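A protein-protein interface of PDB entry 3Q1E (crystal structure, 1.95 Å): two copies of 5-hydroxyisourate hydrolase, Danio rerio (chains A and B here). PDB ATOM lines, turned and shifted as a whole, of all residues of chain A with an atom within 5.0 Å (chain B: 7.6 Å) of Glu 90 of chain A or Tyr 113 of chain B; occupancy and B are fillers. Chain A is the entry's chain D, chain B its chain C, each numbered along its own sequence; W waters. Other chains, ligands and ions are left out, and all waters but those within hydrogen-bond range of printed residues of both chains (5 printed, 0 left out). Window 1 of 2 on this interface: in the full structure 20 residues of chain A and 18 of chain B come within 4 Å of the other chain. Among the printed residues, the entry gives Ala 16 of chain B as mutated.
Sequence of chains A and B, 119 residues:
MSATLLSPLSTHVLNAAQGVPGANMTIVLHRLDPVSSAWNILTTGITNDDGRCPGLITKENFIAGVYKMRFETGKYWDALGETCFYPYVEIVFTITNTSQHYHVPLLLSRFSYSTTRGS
O of Tyr 113 of chain B lies within hydrogen-bond range of N of Thr 115 of chain A (3.0 Å).
The backbone NH (N) of Thr 115 of chain B lies within hydrogen-bond range of the backbone carbonyl oxygen (O) of Tyr 113 of chain A (2.9 Å).
NZ of Lys 68 of chain B is in salt-bridge range of OE2 of Glu 90 of chain B (3.7 Å).
OG1 of Thr 73 of chain B sits close to N of Tyr 88 of chain B (3.3 Å).
The side-chain sulfur of Cys 84 of chain B sits at hydrogen-bond distance from the backbone carbonyl oxygen of Tyr 86 of chain B (3.3 Å).
The side-chain hydroxyl (OG1) of Thr 115 of chain B is in hydrogen-bond range of the backbone carbonyl oxygen (O) of Pro 105 of chain B (2.7 Å).
N of Ser 114 of chain B sits at hydrogen-bond distance from O of Leu 107 of chain B.
OE2 of Glu 90 of chain A is in salt-bridge range of NZ of Lys 68 of chain A (3.4 Å).
OH of Tyr 88 of chain A touches CG2 of Val 92 of chain B, 3.5 Å away.
Tyr 113 of chain B touches Glu 90 of chain A (OH to O, 3.5 Å).
Ile 91 of chain A touches Tyr 86 of chain B (CG2 to CE1, 3.7 Å).
Val 92 of chain A touches Tyr 86 of chain B.
Glu 90 of chain B touches Tyr 113 of chain A.
OH of Tyr 113 of chain A touches CG1 of Ile 91 of chain B (3.7 Å).
CA of Ser 114 of chain B touches O of Tyr 113 of chain A, at 3.3 Å.
O of Tyr 113 of chain B touches CA of Ser 114 of chain A, 3.3 Å away.
CB of Ser 114 of chain B touches CB of Ser 114 of chain A (3.3 Å).
Thr 115 of chain A touches Ser 112 of chain B.
Of the printed residues of chain B, Glu 90 of chain A touches Tyr 113 (3.5 Å).
Of the printed residues of chain B, Tyr 113 of chain A touches Glu 90 (3.6 Å), Ile 91 (3.7 Å), Ser 114 (3.3 Å) and Thr 115 (2.9 Å).
Printed residues of chain A within 4 Å of Ile 91 of chain B: Tyr 113 (3.7 Å).
Pro 105 of chain B touches none of the printed residues of chain A.
Tyr 113 of chain B touches just these residues of chain A: Glu 90 (3.5 Å), Ile 91 (3.9 Å), Ser 114 (3.3 Å) and Thr 115 (3.0 Å).
The nearest printed residue of chain B that does not touch Tyr 88 of chain A is Lys 68 of chain B (4.9 Å).
Printed residues of chain A that touch a printed residue of chain B: Tyr 88, Glu 90, Ile 91, Val 92, Tyr 113, Ser 114 and Thr 115.
Hydrophobic or aromatic side chains of chain A that line the printed part of chain B: Tyr 88, Ile 91, Val 92 and Tyr 113.
Along chain A the printed residues that touch a printed residue of chain B span positions 88 to 115.
Hydrophobic or aromatic side chains of chain B within 4 Å of the printed part of chain A: Tyr 86, Tyr 88, Ile 91, Val 92 and Tyr 113.
Among the printed residues, no Asp or Glu carboxylate lies within 4 Å of a Lys or Arg side-chain nitrogen of the other chain.
Glu 90 of chain A touches Tyr 113 of chain B, and with the chains exchanged Tyr 113 of chain A touches Glu 90 of chain B.
Ile 91 of chain A touches Tyr 113 of chain B, and with the chains exchanged Tyr 113 of chain A touches Ile 91 of chain B.
Tyr 113 of chain A touches Ser 114 of chain B, and with the chains exchanged Ser 114 of chain A touches Tyr 113 of chain B.
Ser 114 of chain B touches its own counterpart, Ser 114 of chain A.
Positions printed for both chains: 68, 88, 89, 90, 91, 92, 113, 114 and 115.
Of the 15 pairs that touch across the chains among the printed residues, 11 have their exchanged pair printed and touching as well.
Water W5 bridges O of Glu 90 of chain A (2.5 Å) and N of Glu 90 of chain B (3.0 Å).
Water W3 lies within hydrogen-bond range of the side-chain hydroxyl (OH) of Tyr 113 of chain A (2.5 Å), the side-chain hydroxyl (OH) of Tyr 113 of chain B (2.6 Å), the backbone carbonyl oxygen (O) of Glu 90 of chain A (3.0 Å) and the backbone carbonyl oxygen (O) of Glu 90 of chain B (3.0 Å).
Water W2 lies within hydrogen-bond range of O of Glu 90 of chain B and N of Glu 90 of chain A.
Water W1 lies within hydrogen-bond range of the backbone carbonyl oxygen (O) of Tyr 88 of chain B (2.8 Å), the backbone NH (N) of Val 92 of chain A (2.9 Å) and the side-chain hydroxyl (OH) of Tyr 113 of chain B (3.1 Å).
Water W4 lies within hydrogen-bond range of OH of Tyr 113 of chain A (3.0 Å), N of Val 92 of chain B (3.0 Å) and O of Tyr 88 of chain A (3.2 Å).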
ATOM      1  N   LYS A  68       3.624 -16.909  10.034  1.00  0.00           N
ATOM      2  CA  LYS A  68       2.219 -16.627  10.257  1.00  0.00           C
ATOM      3  C   LYS A  68       1.683 -17.702  11.195  1.00  0.00           C
ATOM      4  O   LYS A  68       2.048 -18.881  11.043  1.00  0.00           O
ATOM      5  CB  LYS A  68       1.544 -16.586   8.884  1.00  0.00           C
ATOM      6  CG  LYS A  68       0.262 -17.372   8.766  1.00  0.00           C
ATOM      7  CD  LYS A  68      -0.189 -17.431   7.373  1.00  0.00           C
ATOM      8  CE  LYS A  68      -0.707 -18.870   7.077  1.00  0.00           C
ATOM      9  NZ  LYS A  68      -1.286 -18.774   5.750  1.00  0.00           N
ATOM     10  N   MET A  69       0.892 -17.282  12.195  1.00  0.00           N
ATOM     11  CA  MET A  69       0.263 -18.149  13.151  1.00  0.00           C
ATOM     12  C   MET A  69      -1.230 -18.020  12.925  1.00  0.00           C
ATOM     13  O   MET A  69      -1.807 -16.918  12.963  1.00  0.00           O
ATOM     14  CB  MET A  69       0.599 -17.757  14.588  1.00  0.00           C
ATOM     15  CG  MET A  69       1.955 -18.273  15.127  1.00  0.00           C
ATOM     16  SD  MET A  69       2.355 -17.660  16.797  1.00  0.00           S
ATOM     17  CE  MET A  69       1.083 -18.440  17.745  1.00  0.00           C
ATOM     18  N   ARG A  70      -1.850 -19.160  12.693  1.00  0.00           N
ATOM     19  CA  ARG A  70      -3.272 -19.213  12.534  1.00  0.00           C
ATOM     20  C   ARG A  70      -3.850 -19.843  13.793  1.00  0.00           C
ATOM     21  O   ARG A  70      -3.359 -20.891  14.256  1.00  0.00           O
ATOM     22  CB  ARG A  70      -3.624 -20.061  11.324  1.00  0.00           C
ATOM     23  CG  ARG A  70      -5.089 -20.048  10.961  1.00  0.00           C
ATOM     24  CD  ARG A  70      -5.123 -21.068   9.866  1.00  0.00           C
ATOM     25  NE  ARG A  70      -6.388 -21.410   9.271  1.00  0.00           N
ATOM     26  CZ  ARG A  70      -6.702 -21.179   7.989  1.00  0.00           C
ATOM     27  NH1 ARG A  70      -5.864 -20.545   7.154  1.00  0.00           N
ATOM     28  NH2 ARG A  70      -7.870 -21.614   7.547  1.00  0.00           N
ATOM     29  N   TYR A  88     -11.285 -17.781  11.563  1.00  0.00           N
ATOM     30  CA  TYR A  88      -9.966 -18.058  12.084  1.00  0.00           C
ATOM     31  C   TYR A  88      -9.379 -16.683  12.215  1.00  0.00           C
ATOM     32  O   TYR A  88      -9.959 -15.716  11.739  1.00  0.00           O
ATOM     33  CB  TYR A  88      -9.056 -18.928  11.155  1.00  0.00           C
ATOM     34  CG  TYR A  88      -8.739 -18.384   9.756  1.00  0.00           C
ATOM     35  CD1 TYR A  88      -9.442 -18.860   8.667  1.00  0.00           C
ATOM     36  CD2 TYR A  88      -7.736 -17.404   9.526  1.00  0.00           C
ATOM     37  CE1 TYR A  88      -9.206 -18.407   7.391  1.00  0.00           C
ATOM     38  CE2 TYR A  88      -7.498 -16.909   8.206  1.00  0.00           C
ATOM     39  CZ  TYR A  88      -8.238 -17.469   7.151  1.00  0.00           C
ATOM     40  OH  TYR A  88      -8.069 -17.077   5.845  1.00  0.00           O
ATOM     41  N   VAL A  89      -8.264 -16.599  12.903  1.00  0.00           N
ATOM     42  CA  VAL A  89      -7.493 -15.350  12.899  1.00  0.00           C
ATOM     43  C   VAL A  89      -6.124 -15.725  12.464  1.00  0.00           C
ATOM     44  O   VAL A  89      -5.636 -16.722  12.973  1.00  0.00           O
ATOM     45  CB  VAL A  89      -7.467 -14.750  14.321  1.00  0.00           C
ATOM     46  CG1 VAL A  89      -6.288 -13.682  14.437  1.00  0.00           C
ATOM     47  CG2 VAL A  89      -8.887 -14.132  14.666  1.00  0.00           C
ATOM     48  N   GLU A  90      -5.454 -14.918  11.578  1.00  0.00           N
ATOM     49  CA  GLU A  90      -4.041 -15.164  11.243  1.00  0.00           C
ATOM     50  C   GLU A  90      -3.228 -13.914  11.572  1.00  0.00           C
ATOM     51  O   GLU A  90      -3.635 -12.807  11.179  1.00  0.00           O
ATOM     52  CB  GLU A  90      -3.895 -15.478   9.740  1.00  0.00           C
ATOM     53  CG  GLU A  90      -3.828 -16.963   9.426  1.00  0.00           C
ATOM     54  CD  GLU A  90      -3.853 -17.315   7.933  1.00  0.00           C
ATOM     55  OE1 GLU A  90      -3.701 -16.415   7.101  1.00  0.00           O
ATOM     56  OE2 GLU A  90      -4.106 -18.524   7.592  1.00  0.00           O
ATOM     57  N   ILE A  91      -2.113 -14.084  12.290  1.00  0.00           N
ATOM     58  CA  ILE A  91      -1.157 -12.994  12.625  1.00  0.00           C
ATOM     59  C   ILE A  91       0.137 -13.282  11.836  1.00  0.00           C
ATOM     60  O   ILE A  91       0.785 -14.373  11.981  1.00  0.00           O
ATOM     61  CB  ILE A  91      -0.844 -12.985  14.115  1.00  0.00           C
ATOM     62  CG1 ILE A  91      -2.155 -12.906  14.918  1.00  0.00           C
ATOM     63  CG2 ILE A  91      -0.009 -11.755  14.548  1.00  0.00           C
ATOM     64  CD1 ILE A  91      -1.901 -13.020  16.361  1.00  0.00           C
ATOM     65  N   VAL A  92       0.474 -12.339  10.962  1.00  0.00           N
ATOM     66  CA  VAL A  92       1.530 -12.540   9.994  1.00  0.00           C
ATOM     67  C   VAL A  92       2.638 -11.587  10.471  1.00  0.00           C
ATOM     68  O   VAL A  92       2.332 -10.434  10.713  1.00  0.00           O
ATOM     69  CB  VAL A  92       1.051 -12.236   8.516  1.00  0.00           C
ATOM     70  CG1 VAL A  92       2.227 -12.288   7.577  1.00  0.00           C
ATOM     71  CG2 VAL A  92       0.010 -13.336   8.017  1.00  0.00           C
ATOM     72  N   TYR A 113     -10.386  -8.641  18.540  1.00  0.00           N
ATOM     73  CA  TYR A 113      -9.170  -9.273  18.919  1.00  0.00           C
ATOM     74  C   TYR A 113      -8.029  -8.292  18.743  1.00  0.00           C
ATOM     75  O   TYR A 113      -8.113  -7.339  17.980  1.00  0.00           O
ATOM     76  CB  TYR A 113      -8.876 -10.584  18.126  1.00  0.00           C
ATOM     77  CG  TYR A 113      -8.643 -10.508  16.599  1.00  0.00           C
ATOM     78  CD1 TYR A 113      -9.717 -10.644  15.673  1.00  0.00           C
ATOM     79  CD2 TYR A 113      -7.380 -10.348  16.071  1.00  0.00           C
ATOM     80  CE1 TYR A 113      -9.478 -10.591  14.238  1.00  0.00           C
ATOM     81  CE2 TYR A 113      -7.154 -10.287  14.660  1.00  0.00           C
ATOM     82  CZ  TYR A 113      -8.181 -10.425  13.769  1.00  0.00           C
ATOM     83  OH  TYR A 113      -7.917 -10.398  12.419  1.00  0.00           O
ATOM     84  N   SER A 114      -6.970  -8.572  19.449  1.00  0.00           N
ATOM     85  CA  SER A 114      -5.777  -7.738  19.341  1.00  0.00           C
ATOM     86  C   SER A 114      -4.513  -8.567  19.610  1.00  0.00           C
ATOM     87  O   SER A 114      -4.550  -9.667  20.255  1.00  0.00           O
ATOM     88  CB  SER A 114      -5.904  -6.517  20.272  1.00  0.00           C
ATOM     89  OG  SER A 114      -6.001  -6.895  21.611  1.00  0.00           O
ATOM     90  N   THR A 115      -3.403  -8.082  19.063  1.00  0.00           N
ATOM     91  CA  THR A 115      -2.149  -8.747  19.246  1.00  0.00           C
ATOM     92  C   THR A 115      -1.102  -7.650  19.406  1.00  0.00           C
ATOM     93  O   THR A 115      -1.345  -6.488  19.068  1.00  0.00           O
ATOM     94  CB  THR A 115      -1.804  -9.693  18.065  1.00  0.00           C
ATOM     95  OG1 THR A 115      -0.610 -10.410  18.363  1.00  0.00           O
ATOM     96  CG2 THR A 115      -1.605  -8.925  16.719  1.00  0.00           C
ATOM     97  N   ALA B  16      -2.633   4.322  15.740  1.00  0.00           N
ATOM     98  CA  ALA B  16      -2.690   4.418  17.249  1.00  0.00           C
ATOM     99  C   ALA B  16      -1.526   5.081  17.898  1.00  0.00           C
ATOM    100  O   ALA B  16      -1.709   5.597  19.015  1.00  0.00           O
ATOM    101  CB  ALA B  16      -2.885   3.043  17.959  1.00  0.00           C
ATOM    102  N   LYS B  68     -12.805 -11.456   3.372  1.00  0.00           N
ATOM    103  CA  LYS B  68     -11.464 -11.189   3.837  1.00  0.00           C
ATOM    104  C   LYS B  68     -10.988  -9.787   3.395  1.00  0.00           C
ATOM    105  O   LYS B  68     -11.073  -9.403   2.194  1.00  0.00           O
ATOM    106  CB  LYS B  68     -10.496 -12.273   3.362  1.00  0.00           C
ATOM    107  CG  LYS B  68      -9.018 -11.876   3.296  1.00  0.00           C
ATOM    108  CD  LYS B  68      -8.110 -13.072   2.969  1.00  0.00           C
ATOM    109  CE  LYS B  68      -8.006 -13.307   1.475  1.00  0.00           C
ATOM    110  NZ  LYS B  68      -6.668 -13.900   1.085  1.00  0.00           N
ATOM    111  N   THR B  73      -0.231  -3.168   5.547  1.00  0.00           N
ATOM    112  CA  THR B  73       0.350  -2.434   6.653  1.00  0.00           C
ATOM    113  C   THR B  73       1.824  -2.179   6.413  1.00  0.00           C
ATOM    114  O   THR B  73       2.312  -1.086   6.734  1.00  0.00           O
ATOM    115  CB  THR B  73       0.168  -3.187   7.950  1.00  0.00           C
ATOM    116  OG1 THR B  73       0.555  -4.553   7.713  1.00  0.00           O
ATOM    117  CG2 THR B  73      -1.324  -3.149   8.374  1.00  0.00           C
ATOM    118  N   CYS B  84       7.565  -2.122  10.362  1.00  0.00           N
ATOM    119  CA  CYS B  84       6.414  -2.687  11.076  1.00  0.00           C
ATOM    120  C   CYS B  84       6.831  -4.112  11.448  1.00  0.00           C
ATOM    121  O   CYS B  84       7.849  -4.631  10.956  1.00  0.00           O
ATOM    122  CB  CYS B  84       5.122  -2.639  10.197  1.00  0.00           C
ATOM    123  SG  CYS B  84       3.314  -3.109  11.023  1.00  0.00           S
ATOM    124  N   PHE B  85       6.062  -4.754  12.317  1.00  0.00           N
ATOM    125  CA  PHE B  85       6.315  -6.108  12.700  1.00  0.00           C
ATOM    126  C   PHE B  85       5.399  -6.977  11.855  1.00  0.00           C
ATOM    127  O   PHE B  85       5.721  -8.117  11.571  1.00  0.00           O
ATOM    128  CB  PHE B  85       6.005  -6.236  14.209  1.00  0.00           C
ATOM    129  CG  PHE B  85       6.186  -7.630  14.799  1.00  0.00           C
ATOM    130  CD1 PHE B  85       7.405  -8.310  14.692  1.00  0.00           C
ATOM    131  CD2 PHE B  85       5.161  -8.193  15.552  1.00  0.00           C
ATOM    132  CE1 PHE B  85       7.587  -9.565  15.279  1.00  0.00           C
ATOM    133  CE2 PHE B  85       5.306  -9.474  16.169  1.00  0.00           C
ATOM    134  CZ  PHE B  85       6.506 -10.187  16.018  1.00  0.00           C
ATOM    135  N   TYR B  86       4.254  -6.422  11.462  1.00  0.00           N
ATOM    136  CA  TYR B  86       3.280  -7.083  10.582  1.00  0.00           C
ATOM    137  C   TYR B  86       3.320  -6.573   9.125  1.00  0.00           C
ATOM    138  O   TYR B  86       2.844  -5.472   8.805  1.00  0.00           O
ATOM    139  CB  TYR B  86       1.870  -6.885  11.140  1.00  0.00           C
ATOM    140  CG  TYR B  86       1.794  -7.067  12.618  1.00  0.00           C
ATOM    141  CD1 TYR B  86       1.863  -8.340  13.174  1.00  0.00           C
ATOM    142  CD2 TYR B  86       1.744  -5.971  13.477  1.00  0.00           C
ATOM    143  CE1 TYR B  86       1.778  -8.555  14.543  1.00  0.00           C
ATOM    144  CE2 TYR B  86       1.654  -6.185  14.886  1.00  0.00           C
ATOM    145  CZ  TYR B  86       1.680  -7.480  15.385  1.00  0.00           C
ATOM    146  OH  TYR B  86       1.645  -7.763  16.737  1.00  0.00           O
ATOM    147  N   TYR B  88       1.553  -7.474   6.622  1.00  0.00           N
ATOM    148  CA  TYR B  88       0.197  -7.190   6.191  1.00  0.00           C
ATOM    149  C   TYR B  88      -0.713  -7.606   7.319  1.00  0.00           C
ATOM    150  O   TYR B  88      -0.269  -8.267   8.272  1.00  0.00           O
ATOM    151  CB  TYR B  88      -0.154  -7.832   4.832  1.00  0.00           C
ATOM    152  CG  TYR B  88      -0.248  -9.342   4.811  1.00  0.00           C
ATOM    153  CD1 TYR B  88       0.829 -10.121   4.391  1.00  0.00           C
ATOM    154  CD2 TYR B  88      -1.386  -9.982   5.250  1.00  0.00           C
ATOM    155  CE1 TYR B  88       0.777 -11.517   4.396  1.00  0.00           C
ATOM    156  CE2 TYR B  88      -1.451 -11.391   5.265  1.00  0.00           C
ATOM    157  CZ  TYR B  88      -0.366 -12.141   4.804  1.00  0.00           C
ATOM    158  OH  TYR B  88      -0.434 -13.518   4.821  1.00  0.00           O
ATOM    159  N   VAL B  89      -1.973  -7.204   7.222  1.00  0.00           N
ATOM    160  CA  VAL B  89      -2.967  -7.619   8.144  1.00  0.00           C
ATOM    161  C   VAL B  89      -4.164  -8.109   7.328  1.00  0.00           C
ATOM    162  O   VAL B  89      -4.702  -7.375   6.488  1.00  0.00           O
ATOM    163  CB  VAL B  89      -3.336  -6.534   9.198  1.00  0.00           C
ATOM    164  CG1 VAL B  89      -4.617  -7.011  10.019  1.00  0.00           C
ATOM    165  CG2 VAL B  89      -2.110  -6.295  10.163  1.00  0.00           C
ATOM    166  N   GLU B  90      -4.530  -9.380   7.546  1.00  0.00           N
ATOM    167  CA  GLU B  90      -5.803  -9.904   7.009  1.00  0.00           C
ATOM    168  C   GLU B  90      -6.860 -10.160   8.074  1.00  0.00           C
ATOM    169  O   GLU B  90      -6.582 -10.875   9.073  1.00  0.00           O
ATOM    170  CB  GLU B  90      -5.580 -11.182   6.155  1.00  0.00           C
ATOM    171  CG  GLU B  90      -4.997 -10.866   4.743  1.00  0.00           C
ATOM    172  CD  GLU B  90      -4.594 -12.086   3.852  1.00  0.00           C
ATOM    173  OE1 GLU B  90      -4.720 -13.270   4.248  1.00  0.00           O
ATOM    174  OE2 GLU B  90      -4.126 -11.823   2.720  1.00  0.00           O
ATOM    175  N   ILE B  91      -8.081  -9.643   7.839  1.00  0.00           N
ATOM    176  CA  ILE B  91      -9.194  -9.884   8.777  1.00  0.00           C
ATOM    177  C   ILE B  91     -10.210 -10.676   7.995  1.00  0.00           C
ATOM    178  O   ILE B  91     -10.684 -10.217   6.961  1.00  0.00           O
ATOM    179  CB  ILE B  91      -9.877  -8.582   9.312  1.00  0.00           C
ATOM    180  CG1 ILE B  91      -8.852  -7.738  10.076  1.00  0.00           C
ATOM    181  CG2 ILE B  91     -11.127  -8.957  10.148  1.00  0.00           C
ATOM    182  CD1 ILE B  91      -9.288  -6.255  10.397  1.00  0.00           C
ATOM    183  N   VAL B  92     -10.485 -11.877   8.472  1.00  0.00           N
ATOM    184  CA  VAL B  92     -11.446 -12.766   7.820  1.00  0.00           C
ATOM    185  C   VAL B  92     -12.649 -12.862   8.723  1.00  0.00           C
ATOM    186  O   VAL B  92     -12.500 -13.058   9.943  1.00  0.00           O
ATOM    187  CB  VAL B  92     -10.811 -14.140   7.650  1.00  0.00           C
ATOM    188  CG1 VAL B  92     -11.763 -15.128   6.932  1.00  0.00           C
ATOM    189  CG2 VAL B  92      -9.436 -14.011   6.817  1.00  0.00           C
ATOM    190  N   PRO B 105     -12.931  -2.001  11.493  1.00  0.00           N
ATOM    191  CA  PRO B 105     -11.779  -1.082  11.523  1.00  0.00           C
ATOM    192  C   PRO B 105     -10.459  -1.780  11.879  1.00  0.00           C
ATOM    193  O   PRO B 105     -10.416  -3.024  12.198  1.00  0.00           O
ATOM    194  CB  PRO B 105     -12.200  -0.025  12.566  1.00  0.00           C
ATOM    195  CG  PRO B 105     -13.248  -0.717  13.459  1.00  0.00           C
ATOM    196  CD  PRO B 105     -13.698  -1.971  12.766  1.00  0.00           C
ATOM    197  N   LEU B 106      -9.382  -0.997  11.767  1.00  0.00           N
ATOM    198  CA  LEU B 106      -8.056  -1.446  12.106  1.00  0.00           C
ATOM    199  C   LEU B 106      -7.412  -0.296  12.891  1.00  0.00           C
ATOM    200  O   LEU B 106      -7.277   0.777  12.329  1.00  0.00           O
ATOM    201  CB  LEU B 106      -7.224  -1.699  10.867  1.00  0.00           C
ATOM    202  CG  LEU B 106      -5.860  -2.294  11.193  1.00  0.00           C
ATOM    203  CD1 LEU B 106      -5.870  -3.567  12.016  1.00  0.00           C
ATOM    204  CD2 LEU B 106      -5.151  -2.573   9.875  1.00  0.00           C
ATOM    205  N   LEU B 107      -7.092  -0.527  14.170  1.00  0.00           N
ATOM    206  CA  LEU B 107      -6.257   0.352  14.976  1.00  0.00           C
ATOM    207  C   LEU B 107      -4.825  -0.230  14.996  1.00  0.00           C
ATOM    208  O   LEU B 107      -4.604  -1.361  15.422  1.00  0.00           O
ATOM    209  CB  LEU B 107      -6.839   0.328  16.375  1.00  0.00           C
ATOM    210  CG  LEU B 107      -6.076   1.059  17.451  1.00  0.00           C
ATOM    211  CD1 LEU B 107      -6.051   2.523  17.101  1.00  0.00           C
ATOM    212  CD2 LEU B 107      -6.693   0.785  18.881  1.00  0.00           C
ATOM    213  N   LEU B 108      -3.859   0.525  14.526  1.00  0.00           N
ATOM    214  CA  LEU B 108      -2.575  -0.049  14.152  1.00  0.00           C
ATOM    215  C   LEU B 108      -1.442   0.781  14.760  1.00  0.00           C
ATOM    216  O   LEU B 108      -1.510   2.021  14.739  1.00  0.00           O
ATOM    217  CB  LEU B 108      -2.496   0.016  12.590  1.00  0.00           C
ATOM    218  CG  LEU B 108      -1.288  -0.424  11.802  1.00  0.00           C
ATOM    219  CD1 LEU B 108      -1.042  -1.851  12.257  1.00  0.00           C
ATOM    220  CD2 LEU B 108      -1.506  -0.446  10.304  1.00  0.00           C
ATOM    221  N   SER B 109      -0.398   0.139  15.292  1.00  0.00           N
ATOM    222  CA  SER B 109       0.904   0.832  15.521  1.00  0.00           C
ATOM    223  C   SER B 109       1.939   0.043  14.750  1.00  0.00           C
ATOM    224  O   SER B 109       1.585  -0.894  14.036  1.00  0.00           O
ATOM    225  CB  SER B 109       1.250   0.918  17.021  1.00  0.00           C
ATOM    226  OG  SER B 109       2.049  -0.164  17.456  1.00  0.00           O
ATOM    227  N   ARG B 110       3.204   0.347  14.907  1.00  0.00           N
ATOM    228  CA  ARG B 110       4.247  -0.517  14.361  1.00  0.00           C
ATOM    229  C   ARG B 110       4.389  -1.938  14.954  1.00  0.00           C
ATOM    230  O   ARG B 110       4.929  -2.808  14.265  1.00  0.00           O
ATOM    231  CB  ARG B 110       5.595   0.173  14.484  1.00  0.00           C
ATOM    232  CG  ARG B 110       5.663   1.411  13.689  1.00  0.00           C
ATOM    233  CD  ARG B 110       7.127   1.586  13.291  1.00  0.00           C
ATOM    234  NE  ARG B 110       7.961   1.959  14.393  1.00  0.00           N
ATOM    235  CZ  ARG B 110       9.213   1.547  14.605  1.00  0.00           C
ATOM    236  NH1 ARG B 110       9.787   0.658  13.801  1.00  0.00           N
ATOM    237  NH2 ARG B 110       9.866   2.006  15.671  1.00  0.00           N
ATOM    238  N   PHE B 111       3.915  -2.170  16.197  1.00  0.00           N
ATOM    239  CA  PHE B 111       4.025  -3.484  16.881  1.00  0.00           C
ATOM    240  C   PHE B 111       2.739  -4.004  17.513  1.00  0.00           C
ATOM    241  O   PHE B 111       2.784  -4.947  18.344  1.00  0.00           O
ATOM    242  CB  PHE B 111       5.087  -3.388  17.973  1.00  0.00           C
ATOM    243  CG  PHE B 111       6.439  -3.027  17.437  1.00  0.00           C
ATOM    244  CD1 PHE B 111       7.287  -4.024  16.932  1.00  0.00           C
ATOM    245  CD2 PHE B 111       6.842  -1.700  17.383  1.00  0.00           C
ATOM    246  CE1 PHE B 111       8.560  -3.685  16.411  1.00  0.00           C
ATOM    247  CE2 PHE B 111       8.112  -1.343  16.881  1.00  0.00           C
ATOM    248  CZ  PHE B 111       8.964  -2.341  16.398  1.00  0.00           C
ATOM    249  N   SER B 112       1.620  -3.376  17.193  1.00  0.00           N
ATOM    250  CA  SER B 112       0.361  -3.876  17.732  1.00  0.00           C
ATOM    251  C   SER B 112      -0.761  -3.534  16.788  1.00  0.00           C
ATOM    252  O   SER B 112      -0.633  -2.635  15.928  1.00  0.00           O
ATOM    253  CB  SER B 112       0.102  -3.362  19.185  1.00  0.00           C
ATOM    254  OG  SER B 112      -0.582  -2.168  19.173  1.00  0.00           O
ATOM    255  N   TYR B 113      -1.837  -4.303  16.871  1.00  0.00           N
ATOM    256  CA  TYR B 113      -3.029  -3.964  16.140  1.00  0.00           C
ATOM    257  C   TYR B 113      -4.235  -4.548  16.795  1.00  0.00           C
ATOM    258  O   TYR B 113      -4.131  -5.547  17.532  1.00  0.00           O
ATOM    259  CB  TYR B 113      -2.951  -4.313  14.654  1.00  0.00           C
ATOM    260  CG  TYR B 113      -3.001  -5.803  14.168  1.00  0.00           C
ATOM    261  CD1 TYR B 113      -1.811  -6.532  13.924  1.00  0.00           C
ATOM    262  CD2 TYR B 113      -4.192  -6.422  13.891  1.00  0.00           C
ATOM    263  CE1 TYR B 113      -1.845  -7.864  13.439  1.00  0.00           C
ATOM    264  CE2 TYR B 113      -4.224  -7.712  13.402  1.00  0.00           C
ATOM    265  CZ  TYR B 113      -3.053  -8.416  13.173  1.00  0.00           C
ATOM    266  OH  TYR B 113      -3.119  -9.664  12.687  1.00  0.00           O
ATOM    267  N   SER B 114      -5.376  -3.981  16.493  1.00  0.00           N
ATOM    268  CA  SER B 114      -6.647  -4.557  17.007  1.00  0.00           C
ATOM    269  C   SER B 114      -7.797  -4.306  16.051  1.00  0.00           C
ATOM    270  O   SER B 114      -7.767  -3.368  15.231  1.00  0.00           O
ATOM    271  CB  SER B 114      -6.948  -3.995  18.408  1.00  0.00           C
ATOM    272  OG  SER B 114      -7.628  -2.794  18.299  1.00  0.00           O
ATOM    273  N   THR B 115      -8.807  -5.175  16.111  1.00  0.00           N
ATOM    274  CA  THR B 115      -9.993  -4.958  15.331  1.00  0.00           C
ATOM    275  C   THR B 115     -11.254  -5.318  16.115  1.00  0.00           C
ATOM    276  O   THR B 115     -11.200  -6.092  17.085  1.00  0.00           O
ATOM    277  CB  THR B 115      -9.928  -5.718  13.973  1.00  0.00           C
ATOM    278  OG1 THR B 115     -11.087  -5.409  13.206  1.00  0.00           O
ATOM    279  CG2 THR B 115      -9.857  -7.206  14.189  1.00  0.00           C
HETATM  280  O   HOH W   1      -1.098  -9.973  10.390  1.00  0.00           O
HETATM  281  O   HOH W   2      -6.948 -13.390   9.635  1.00  0.00           O
HETATM  282  O   HOH W   3      -5.446 -10.480  11.849  1.00  0.00           O
HETATM  283  O   HOH W   4      -9.229 -12.693  11.068  1.00  0.00           O
HETATM  284  O   HOH W   5      -3.071 -11.427   9.126  1.00  0.00           O
